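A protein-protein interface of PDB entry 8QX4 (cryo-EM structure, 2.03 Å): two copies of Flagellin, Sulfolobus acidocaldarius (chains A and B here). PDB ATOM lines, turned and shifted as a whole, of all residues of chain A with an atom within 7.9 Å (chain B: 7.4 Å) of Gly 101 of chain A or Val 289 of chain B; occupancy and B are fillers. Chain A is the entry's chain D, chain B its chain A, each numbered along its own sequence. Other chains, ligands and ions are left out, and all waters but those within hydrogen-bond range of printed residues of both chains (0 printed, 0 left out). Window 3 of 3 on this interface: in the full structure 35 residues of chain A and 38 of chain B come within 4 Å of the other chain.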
ATOM      1  N   PHE A  95      11.148  38.717  20.025  1.00  0.00           N
ATOM      2  CA  PHE A  95      12.278  39.004  19.159  1.00  0.00           C
ATOM      3  C   PHE A  95      13.309  37.884  19.294  1.00  0.00           C
ATOM      4  O   PHE A  95      13.754  37.593  20.401  1.00  0.00           O
ATOM      5  CB  PHE A  95      12.884  40.363  19.521  1.00  0.00           C
ATOM      6  CG  PHE A  95      14.072  40.740  18.673  1.00  0.00           C
ATOM      7  CD1 PHE A  95      15.349  40.294  18.993  1.00  0.00           C
ATOM      8  CD2 PHE A  95      13.911  41.528  17.542  1.00  0.00           C
ATOM      9  CE1 PHE A  95      16.439  40.630  18.202  1.00  0.00           C
ATOM     10  CE2 PHE A  95      15.004  41.875  16.759  1.00  0.00           C
ATOM     11  CZ  PHE A  95      16.261  41.414  17.082  1.00  0.00           C
ATOM     12  N   THR A  96      13.697  37.261  18.172  1.00  0.00           N
ATOM     13  CA  THR A  96      14.711  36.209  18.207  1.00  0.00           C
ATOM     14  C   THR A  96      15.762  36.407  17.112  1.00  0.00           C
ATOM     15  O   THR A  96      15.451  36.800  15.990  1.00  0.00           O
ATOM     16  CB  THR A  96      14.121  34.785  18.210  1.00  0.00           C
ATOM     17  OG1 THR A  96      13.793  34.369  16.885  1.00  0.00           O
ATOM     18  CG2 THR A  96      12.922  34.597  19.116  1.00  0.00           C
ATOM     19  N   ALA A  97      17.020  36.134  17.470  1.00  0.00           N
ATOM     20  CA  ALA A  97      18.125  36.054  16.530  1.00  0.00           C
ATOM     21  C   ALA A  97      18.821  34.720  16.783  1.00  0.00           C
ATOM     22  O   ALA A  97      19.753  34.642  17.582  1.00  0.00           O
ATOM     23  CB  ALA A  97      19.032  37.258  16.692  1.00  0.00           C
ATOM     24  N   ALA A  98      18.306  33.676  16.122  1.00  0.00           N
ATOM     25  CA  ALA A  98      18.566  32.276  16.436  1.00  0.00           C
ATOM     26  C   ALA A  98      20.060  31.940  16.400  1.00  0.00           C
ATOM     27  O   ALA A  98      20.566  31.267  17.302  1.00  0.00           O
ATOM     28  CB  ALA A  98      17.757  31.402  15.507  1.00  0.00           C
ATOM     29  N   SER A  99      20.766  32.464  15.385  1.00  0.00           N
ATOM     30  CA  SER A  99      22.183  32.215  15.136  1.00  0.00           C
ATOM     31  C   SER A  99      23.055  32.535  16.354  1.00  0.00           C
ATOM     32  O   SER A  99      24.019  31.817  16.623  1.00  0.00           O
ATOM     33  CB  SER A  99      22.655  32.965  13.913  1.00  0.00           C
ATOM     34  OG  SER A  99      21.750  32.797  12.828  1.00  0.00           O
ATOM     35  N   ARG A 100      22.712  33.609  17.085  1.00  0.00           N
ATOM     36  CA  ARG A 100      23.451  34.059  18.261  1.00  0.00           C
ATOM     37  C   ARG A 100      22.754  33.705  19.582  1.00  0.00           C
ATOM     38  O   ARG A 100      23.204  34.129  20.649  1.00  0.00           O
ATOM     39  CB  ARG A 100      23.765  35.559  18.161  1.00  0.00           C
ATOM     40  CG  ARG A 100      22.544  36.470  18.184  1.00  0.00           C
ATOM     41  CD  ARG A 100      22.935  37.931  18.299  1.00  0.00           C
ATOM     42  NE  ARG A 100      23.561  38.405  17.072  1.00  0.00           N
ATOM     43  CZ  ARG A 100      24.152  39.585  16.906  1.00  0.00           C
ATOM     44  NH1 ARG A 100      24.676  39.884  15.730  1.00  0.00           N
ATOM     45  NH2 ARG A 100      24.212  40.456  17.898  1.00  0.00           N
ATOM     46  N   GLY A 101      21.652  32.943  19.520  1.00  0.00           N
ATOM     47  CA  GLY A 101      20.975  32.436  20.706  1.00  0.00           C
ATOM     48  C   GLY A 101      20.195  33.495  21.487  1.00  0.00           C
ATOM     49  O   GLY A 101      19.820  33.250  22.633  1.00  0.00           O
ATOM     50  N   VAL A 102      19.941  34.662  20.878  1.00  0.00           N
ATOM     51  CA  VAL A 102      19.085  35.674  21.489  1.00  0.00           C
ATOM     52  C   VAL A 102      17.626  35.277  21.263  1.00  0.00           C
ATOM     53  O   VAL A 102      17.208  35.047  20.130  1.00  0.00           O
ATOM     54  CB  VAL A 102      19.392  37.094  20.964  1.00  0.00           C
ATOM     55  CG1 VAL A 102      18.285  38.096  21.275  1.00  0.00           C
ATOM     56  CG2 VAL A 102      20.725  37.602  21.488  1.00  0.00           C
ATOM     57  N   SER A 103      16.859  35.211  22.357  1.00  0.00           N
ATOM     58  CA  SER A 103      15.444  34.892  22.290  1.00  0.00           C
ATOM     59  C   SER A 103      14.703  35.613  23.411  1.00  0.00           C
ATOM     60  O   SER A 103      14.871  35.274  24.578  1.00  0.00           O
ATOM     61  CB  SER A 103      15.226  33.401  22.351  1.00  0.00           C
ATOM     62  OG  SER A 103      13.839  33.112  22.348  1.00  0.00           O
ATOM     63  N   LEU A 104      13.899  36.613  23.030  1.00  0.00           N
ATOM     64  CA  LEU A 104      13.113  37.410  23.959  1.00  0.00           C
ATOM     65  C   LEU A 104      11.641  37.090  23.720  1.00  0.00           C
ATOM     66  O   LEU A 104      11.138  37.255  22.611  1.00  0.00           O
ATOM     67  CB  LEU A 104      13.418  38.898  23.737  1.00  0.00           C
ATOM     68  CG  LEU A 104      14.898  39.292  23.744  1.00  0.00           C
ATOM     69  CD1 LEU A 104      15.081  40.741  23.321  1.00  0.00           C
ATOM     70  CD2 LEU A 104      15.535  39.050  25.104  1.00  0.00           C
ATOM     71  N   GLU A 262      22.825  36.735   9.306  1.00  0.00           N
ATOM     72  CA  GLU A 262      21.996  36.200  10.378  1.00  0.00           C
ATOM     73  C   GLU A 262      20.515  36.364  10.040  1.00  0.00           C
ATOM     74  O   GLU A 262      20.125  37.312   9.364  1.00  0.00           O
ATOM     75  CB  GLU A 262      22.261  36.984  11.664  1.00  0.00           C
ATOM     76  CG  GLU A 262      23.495  36.526  12.412  1.00  0.00           C
ATOM     77  CD  GLU A 262      23.871  37.429  13.572  1.00  0.00           C
ATOM     78  OE1 GLU A 262      24.237  38.595  13.319  1.00  0.00           O
ATOM     79  OE2 GLU A 262      23.786  36.976  14.730  1.00  0.00           O
ATOM     80  N   VAL B  56       8.650  26.789  17.579  1.00  0.00           N
ATOM     81  CA  VAL B  56       9.340  25.913  18.514  1.00  0.00           C
ATOM     82  C   VAL B  56      10.845  26.099  18.325  1.00  0.00           C
ATOM     83  O   VAL B  56      11.365  25.898  17.230  1.00  0.00           O
ATOM     84  CB  VAL B  56       8.932  24.433  18.350  1.00  0.00           C
ATOM     85  CG1 VAL B  56       9.608  23.552  19.389  1.00  0.00           C
ATOM     86  CG2 VAL B  56       7.422  24.237  18.409  1.00  0.00           C
ATOM     87  N   LEU B  57      11.529  26.473  19.414  1.00  0.00           N
ATOM     88  CA  LEU B  57      12.960  26.742  19.431  1.00  0.00           C
ATOM     89  C   LEU B  57      13.693  25.594  20.119  1.00  0.00           C
ATOM     90  O   LEU B  57      13.222  25.071  21.126  1.00  0.00           O
ATOM     91  CB  LEU B  57      13.221  28.053  20.182  1.00  0.00           C
ATOM     92  CG  LEU B  57      12.489  29.295  19.671  1.00  0.00           C
ATOM     93  CD1 LEU B  57      12.891  30.517  20.476  1.00  0.00           C
ATOM     94  CD2 LEU B  57      12.755  29.528  18.192  1.00  0.00           C
ATOM     95  N   TYR B  58      14.877  25.250  19.598  1.00  0.00           N
ATOM     96  CA  TYR B  58      15.679  24.141  20.092  1.00  0.00           C
ATOM     97  C   TYR B  58      17.127  24.609  20.268  1.00  0.00           C
ATOM     98  O   TYR B  58      17.636  25.316  19.411  1.00  0.00           O
ATOM     99  CB  TYR B  58      15.517  22.962  19.124  1.00  0.00           C
ATOM    100  CG  TYR B  58      16.374  21.752  19.392  1.00  0.00           C
ATOM    101  CD1 TYR B  58      16.535  21.268  20.679  1.00  0.00           C
ATOM    102  CD2 TYR B  58      16.987  21.058  18.354  1.00  0.00           C
ATOM    103  CE1 TYR B  58      17.308  20.149  20.937  1.00  0.00           C
ATOM    104  CE2 TYR B  58      17.766  19.934  18.597  1.00  0.00           C
ATOM    105  CZ  TYR B  58      17.926  19.477  19.896  1.00  0.00           C
ATOM    106  OH  TYR B  58      18.701  18.385  20.176  1.00  0.00           O
ATOM    107  N   ALA B  59      17.790  24.221  21.370  1.00  0.00           N
ATOM    108  CA  ALA B  59      19.132  24.694  21.703  1.00  0.00           C
ATOM    109  C   ALA B  59      20.092  23.527  21.948  1.00  0.00           C
ATOM    110  O   ALA B  59      19.755  22.580  22.657  1.00  0.00           O
ATOM    111  CB  ALA B  59      19.065  25.598  22.908  1.00  0.00           C
ATOM    112  N   VAL B  60      21.322  23.647  21.414  1.00  0.00           N
ATOM    113  CA  VAL B  60      22.340  22.599  21.433  1.00  0.00           C
ATOM    114  C   VAL B  60      23.727  23.224  21.623  1.00  0.00           C
ATOM    115  O   VAL B  60      23.884  24.433  21.468  1.00  0.00           O
ATOM    116  CB  VAL B  60      22.287  21.737  20.150  1.00  0.00           C
ATOM    117  CG1 VAL B  60      20.930  21.079  19.935  1.00  0.00           C
ATOM    118  CG2 VAL B  60      22.691  22.504  18.896  1.00  0.00           C
ATOM    119  N   TYR B  62      26.151  23.981  19.910  1.00  0.00           N
ATOM    120  CA  TYR B  62      26.594  24.367  18.581  1.00  0.00           C
ATOM    121  C   TYR B  62      27.959  25.056  18.635  1.00  0.00           C
ATOM    122  O   TYR B  62      28.221  25.817  19.570  1.00  0.00           O
ATOM    123  CB  TYR B  62      25.545  25.320  18.012  1.00  0.00           C
ATOM    124  CG  TYR B  62      25.721  25.666  16.561  1.00  0.00           C
ATOM    125  CD1 TYR B  62      25.161  24.868  15.574  1.00  0.00           C
ATOM    126  CD2 TYR B  62      26.469  26.772  16.178  1.00  0.00           C
ATOM    127  CE1 TYR B  62      25.302  25.186  14.234  1.00  0.00           C
ATOM    128  CE2 TYR B  62      26.618  27.101  14.838  1.00  0.00           C
ATOM    129  CZ  TYR B  62      26.025  26.307  13.867  1.00  0.00           C
ATOM    130  OH  TYR B  62      26.112  26.593  12.536  1.00  0.00           O
ATOM    131  N   TRP B  70      17.924  22.605  25.623  1.00  0.00           N
ATOM    132  CA  TRP B  70      16.531  22.911  25.918  1.00  0.00           C
ATOM    133  C   TRP B  70      15.683  23.081  24.662  1.00  0.00           C
ATOM    134  O   TRP B  70      16.204  23.286  23.574  1.00  0.00           O
ATOM    135  CB  TRP B  70      16.391  24.137  26.829  1.00  0.00           C
ATOM    136  CG  TRP B  70      17.118  25.389  26.441  1.00  0.00           C
ATOM    137  CD1 TRP B  70      18.277  25.841  27.002  1.00  0.00           C
ATOM    138  CD2 TRP B  70      16.710  26.410  25.499  1.00  0.00           C
ATOM    139  NE1 TRP B  70      18.626  27.052  26.464  1.00  0.00           N
ATOM    140  CE2 TRP B  70      17.684  27.436  25.543  1.00  0.00           C
ATOM    141  CE3 TRP B  70      15.627  26.570  24.620  1.00  0.00           C
ATOM    142  CZ2 TRP B  70      17.611  28.578  24.732  1.00  0.00           C
ATOM    143  CZ3 TRP B  70      15.543  27.699  23.827  1.00  0.00           C
ATOM    144  CH2 TRP B  70      16.527  28.691  23.882  1.00  0.00           C
ATOM    145  N   TYR B  72      12.031  25.450  23.696  1.00  0.00           N
ATOM    146  CA  TYR B  72      11.111  26.489  24.132  1.00  0.00           C
ATOM    147  C   TYR B  72       9.997  26.622  23.095  1.00  0.00           C
ATOM    148  O   TYR B  72      10.269  26.594  21.901  1.00  0.00           O
ATOM    149  CB  TYR B  72      11.852  27.813  24.392  1.00  0.00           C
ATOM    150  CG  TYR B  72      10.901  28.962  24.606  1.00  0.00           C
ATOM    151  CD1 TYR B  72      10.358  29.218  25.860  1.00  0.00           C
ATOM    152  CD2 TYR B  72      10.475  29.742  23.539  1.00  0.00           C
ATOM    153  CE1 TYR B  72       9.421  30.223  26.050  1.00  0.00           C
ATOM    154  CE2 TYR B  72       9.547  30.757  23.713  1.00  0.00           C
ATOM    155  CZ  TYR B  72       9.011  30.990  24.970  1.00  0.00           C
ATOM    156  OH  TYR B  72       8.073  31.973  25.116  1.00  0.00           O
ATOM    157  N   ASN B 155      15.611  33.606  29.980  1.00  0.00           N
ATOM    158  CA  ASN B 155      16.720  33.765  30.918  1.00  0.00           C
ATOM    159  C   ASN B 155      16.248  34.280  32.280  1.00  0.00           C
ATOM    160  O   ASN B 155      16.612  33.721  33.316  1.00  0.00           O
ATOM    161  CB  ASN B 155      17.826  34.632  30.322  1.00  0.00           C
ATOM    162  CG  ASN B 155      18.283  34.120  28.974  1.00  0.00           C
ATOM    163  OD1 ASN B 155      18.643  32.954  28.829  1.00  0.00           O
ATOM    164  ND2 ASN B 155      18.245  34.981  27.974  1.00  0.00           N
ATOM    165  N   PHE B 202      23.906  30.865  29.772  1.00  0.00           N
ATOM    166  CA  PHE B 202      23.206  32.008  29.212  1.00  0.00           C
ATOM    167  C   PHE B 202      23.769  33.297  29.807  1.00  0.00           C
ATOM    168  O   PHE B 202      24.326  33.283  30.902  1.00  0.00           O
ATOM    169  CB  PHE B 202      21.700  31.877  29.448  1.00  0.00           C
ATOM    170  CG  PHE B 202      21.257  31.925  30.890  1.00  0.00           C
ATOM    171  CD1 PHE B 202      21.180  30.766  31.655  1.00  0.00           C
ATOM    172  CD2 PHE B 202      20.902  33.127  31.484  1.00  0.00           C
ATOM    173  CE1 PHE B 202      20.762  30.815  32.980  1.00  0.00           C
ATOM    174  CE2 PHE B 202      20.484  33.176  32.807  1.00  0.00           C
ATOM    175  CZ  PHE B 202      20.411  32.019  33.552  1.00  0.00           C
ATOM    176  N   PRO B 285      20.555  20.765  13.483  1.00  0.00           N
ATOM    177  CA  PRO B 285      20.457  22.123  14.017  1.00  0.00           C
ATOM    178  C   PRO B 285      21.526  23.041  13.431  1.00  0.00           C
ATOM    179  O   PRO B 285      22.685  22.645  13.300  1.00  0.00           O
ATOM    180  CB  PRO B 285      20.648  21.927  15.527  1.00  0.00           C
ATOM    181  CG  PRO B 285      21.527  20.705  15.641  1.00  0.00           C
ATOM    182  CD  PRO B 285      21.128  19.831  14.468  1.00  0.00           C
ATOM    183  N   ASP B 286      21.129  24.291  13.144  1.00  0.00           N
ATOM    184  CA  ASP B 286      21.886  25.187  12.275  1.00  0.00           C
ATOM    185  C   ASP B 286      22.538  26.374  12.999  1.00  0.00           C
ATOM    186  O   ASP B 286      23.295  27.123  12.376  1.00  0.00           O
ATOM    187  CB  ASP B 286      21.045  25.615  11.066  1.00  0.00           C
ATOM    188  CG  ASP B 286      19.699  26.249  11.386  1.00  0.00           C
ATOM    189  OD1 ASP B 286      19.383  26.428  12.580  1.00  0.00           O
ATOM    190  OD2 ASP B 286      18.966  26.557  10.426  1.00  0.00           O
ATOM    191  N   GLY B 287      22.256  26.534  14.306  1.00  0.00           N
ATOM    192  CA  GLY B 287      22.796  27.598  15.147  1.00  0.00           C
ATOM    193  C   GLY B 287      22.648  27.291  16.640  1.00  0.00           C
ATOM    194  O   GLY B 287      22.098  26.252  17.004  1.00  0.00           O
ATOM    195  N   LYS B 288      23.112  28.219  17.497  1.00  0.00           N
ATOM    196  CA  LYS B 288      23.021  28.101  18.951  1.00  0.00           C
ATOM    197  C   LYS B 288      21.583  27.813  19.384  1.00  0.00           C
ATOM    198  O   LYS B 288      21.356  27.011  20.289  1.00  0.00           O
ATOM    199  CB  LYS B 288      23.539  29.366  19.638  1.00  0.00           C
ATOM    200  CG  LYS B 288      25.044  29.423  19.828  1.00  0.00           C
ATOM    201  CD  LYS B 288      25.467  30.596  20.674  1.00  0.00           C
ATOM    202  CE  LYS B 288      26.965  30.670  20.869  1.00  0.00           C
ATOM    203  NZ  LYS B 288      27.350  31.816  21.728  1.00  0.00           N
ATOM    204  N   VAL B 289      20.634  28.513  18.751  1.00  0.00           N
ATOM    205  CA  VAL B 289      19.222  28.169  18.767  1.00  0.00           C
ATOM    206  C   VAL B 289      18.820  27.872  17.322  1.00  0.00           C
ATOM    207  O   VAL B 289      19.318  28.506  16.396  1.00  0.00           O
ATOM    208  CB  VAL B 289      18.379  29.291  19.408  1.00  0.00           C
ATOM    209  CG1 VAL B 289      16.884  29.087  19.215  1.00  0.00           C
ATOM    210  CG2 VAL B 289      18.696  29.452  20.886  1.00  0.00           C
ATOM    211  N   THR B 290      17.935  26.884  17.134  1.00  0.00           N
ATOM    212  CA  THR B 290      17.417  26.531  15.819  1.00  0.00           C
ATOM    213  C   THR B 290      15.891  26.499  15.873  1.00  0.00           C
ATOM    214  O   THR B 290      15.316  26.116  16.885  1.00  0.00           O
ATOM    215  CB  THR B 290      18.059  25.235  15.305  1.00  0.00           C
ATOM    216  OG1 THR B 290      17.676  25.037  13.945  1.00  0.00           O
ATOM    217  CG2 THR B 290      17.693  23.998  16.098  1.00  0.00           C
ATOM    218  N   VAL B 291      15.242  26.915  14.780  1.00  0.00           N
ATOM    219  CA  VAL B 291      13.790  26.927  14.695  1.00  0.00           C
ATOM    220  C   VAL B 291      13.343  25.598  14.086  1.00  0.00           C
ATOM    221  O   VAL B 291      13.622  25.335  12.918  1.00  0.00           O
ATOM    222  CB  VAL B 291      13.295  28.136  13.874  1.00  0.00           C
ATOM    223  CG1 VAL B 291      11.791  28.114  13.672  1.00  0.00           C
ATOM    224  CG2 VAL B 291      13.729  29.461  14.480  1.00  0.00           C
ATOM    225  N   ILE B 292      12.618  24.780  14.865  1.00  0.00           N
ATOM    226  CA  ILE B 292      12.281  23.424  14.437  1.00  0.00           C
ATOM    227  C   ILE B 292      10.812  23.279  14.026  1.00  0.00           C
ATOM    228  O   ILE B 292      10.474  22.313  13.342  1.00  0.00           O
ATOM    229  CB  ILE B 292      12.708  22.342  15.457  1.00  0.00           C
ATOM    230  CG1 ILE B 292      12.004  22.486  16.813  1.00  0.00           C
ATOM    231  CG2 ILE B 292      14.226  22.291  15.579  1.00  0.00           C
ATOM    232  CD1 ILE B 292      12.104  21.261  17.699  1.00  0.00           C
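The backbone carbonyl oxygen (O) of Ala 98 of chain A sits at hydrogen-bond distance from the backbone NH (N) of Val 289 of chain B, at 3.1 Å.
The backbone NH of Leu 57 of chain B is in hydrogen-bond range of the backbone carbonyl oxygen of Tyr 72 of chain B, at 2.8 Å.
Ala 98 of chain A touches Lys 288 of chain B (O to N, 3.98 Å).
Lys 288 of chain B touches Ser 99 of chain A (N to O, 3.8 Å).
CA of Gly 101 of chain A touches CG2 of Val 289 of chain B, 3.8 Å away.
Ser 103 of chain A touches Leu 57 of chain B (OG to CD1, 3.3 Å).
Of the printed residues of chain B, Ala 98 of chain A touches Lys 288 (3.98 Å) and Val 289 (3.1 Å).
Of the printed residues of chain B, Ser 99 of chain A touches Lys 288.
Gly 101 of chain A touches one residue of chain B.
Of the printed residues of chain B, Ser 103 of chain A touches Leu 57 (3.3 Å).
Printed residues of chain A within 4 Å of Leu 57 of chain B: Ser 103.
Printed residues of chain A within 4 Å of Lys 288 of chain B: Ala 98 and Ser 99.
Val 289 of chain B touches just these residues of chain A: Ala 98 (3.1 Å) and Gly 101 (3.8 Å).
The nearest residue of chain A that does not touch Val 289 of chain B is Ser 99 of chain A (4.3 Å).
Hydrophobic or aromatic side chains of chain A that line the printed part of chain B: Ala 98.
Printed residues of chain B that touch a printed residue of chain A: Leu 57, Lys 288 and Val 289.
Hydrophobic or aromatic side chains of chain B that line the printed part of chain A: Leu 57 and Val 289.
Among the printed residues, 5 pairs touch across the chains.
No position is printed for both chains.
Of the 5 pairs that touch across the chains among the printed residues, none has its exchanged pair printed and touching as well.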
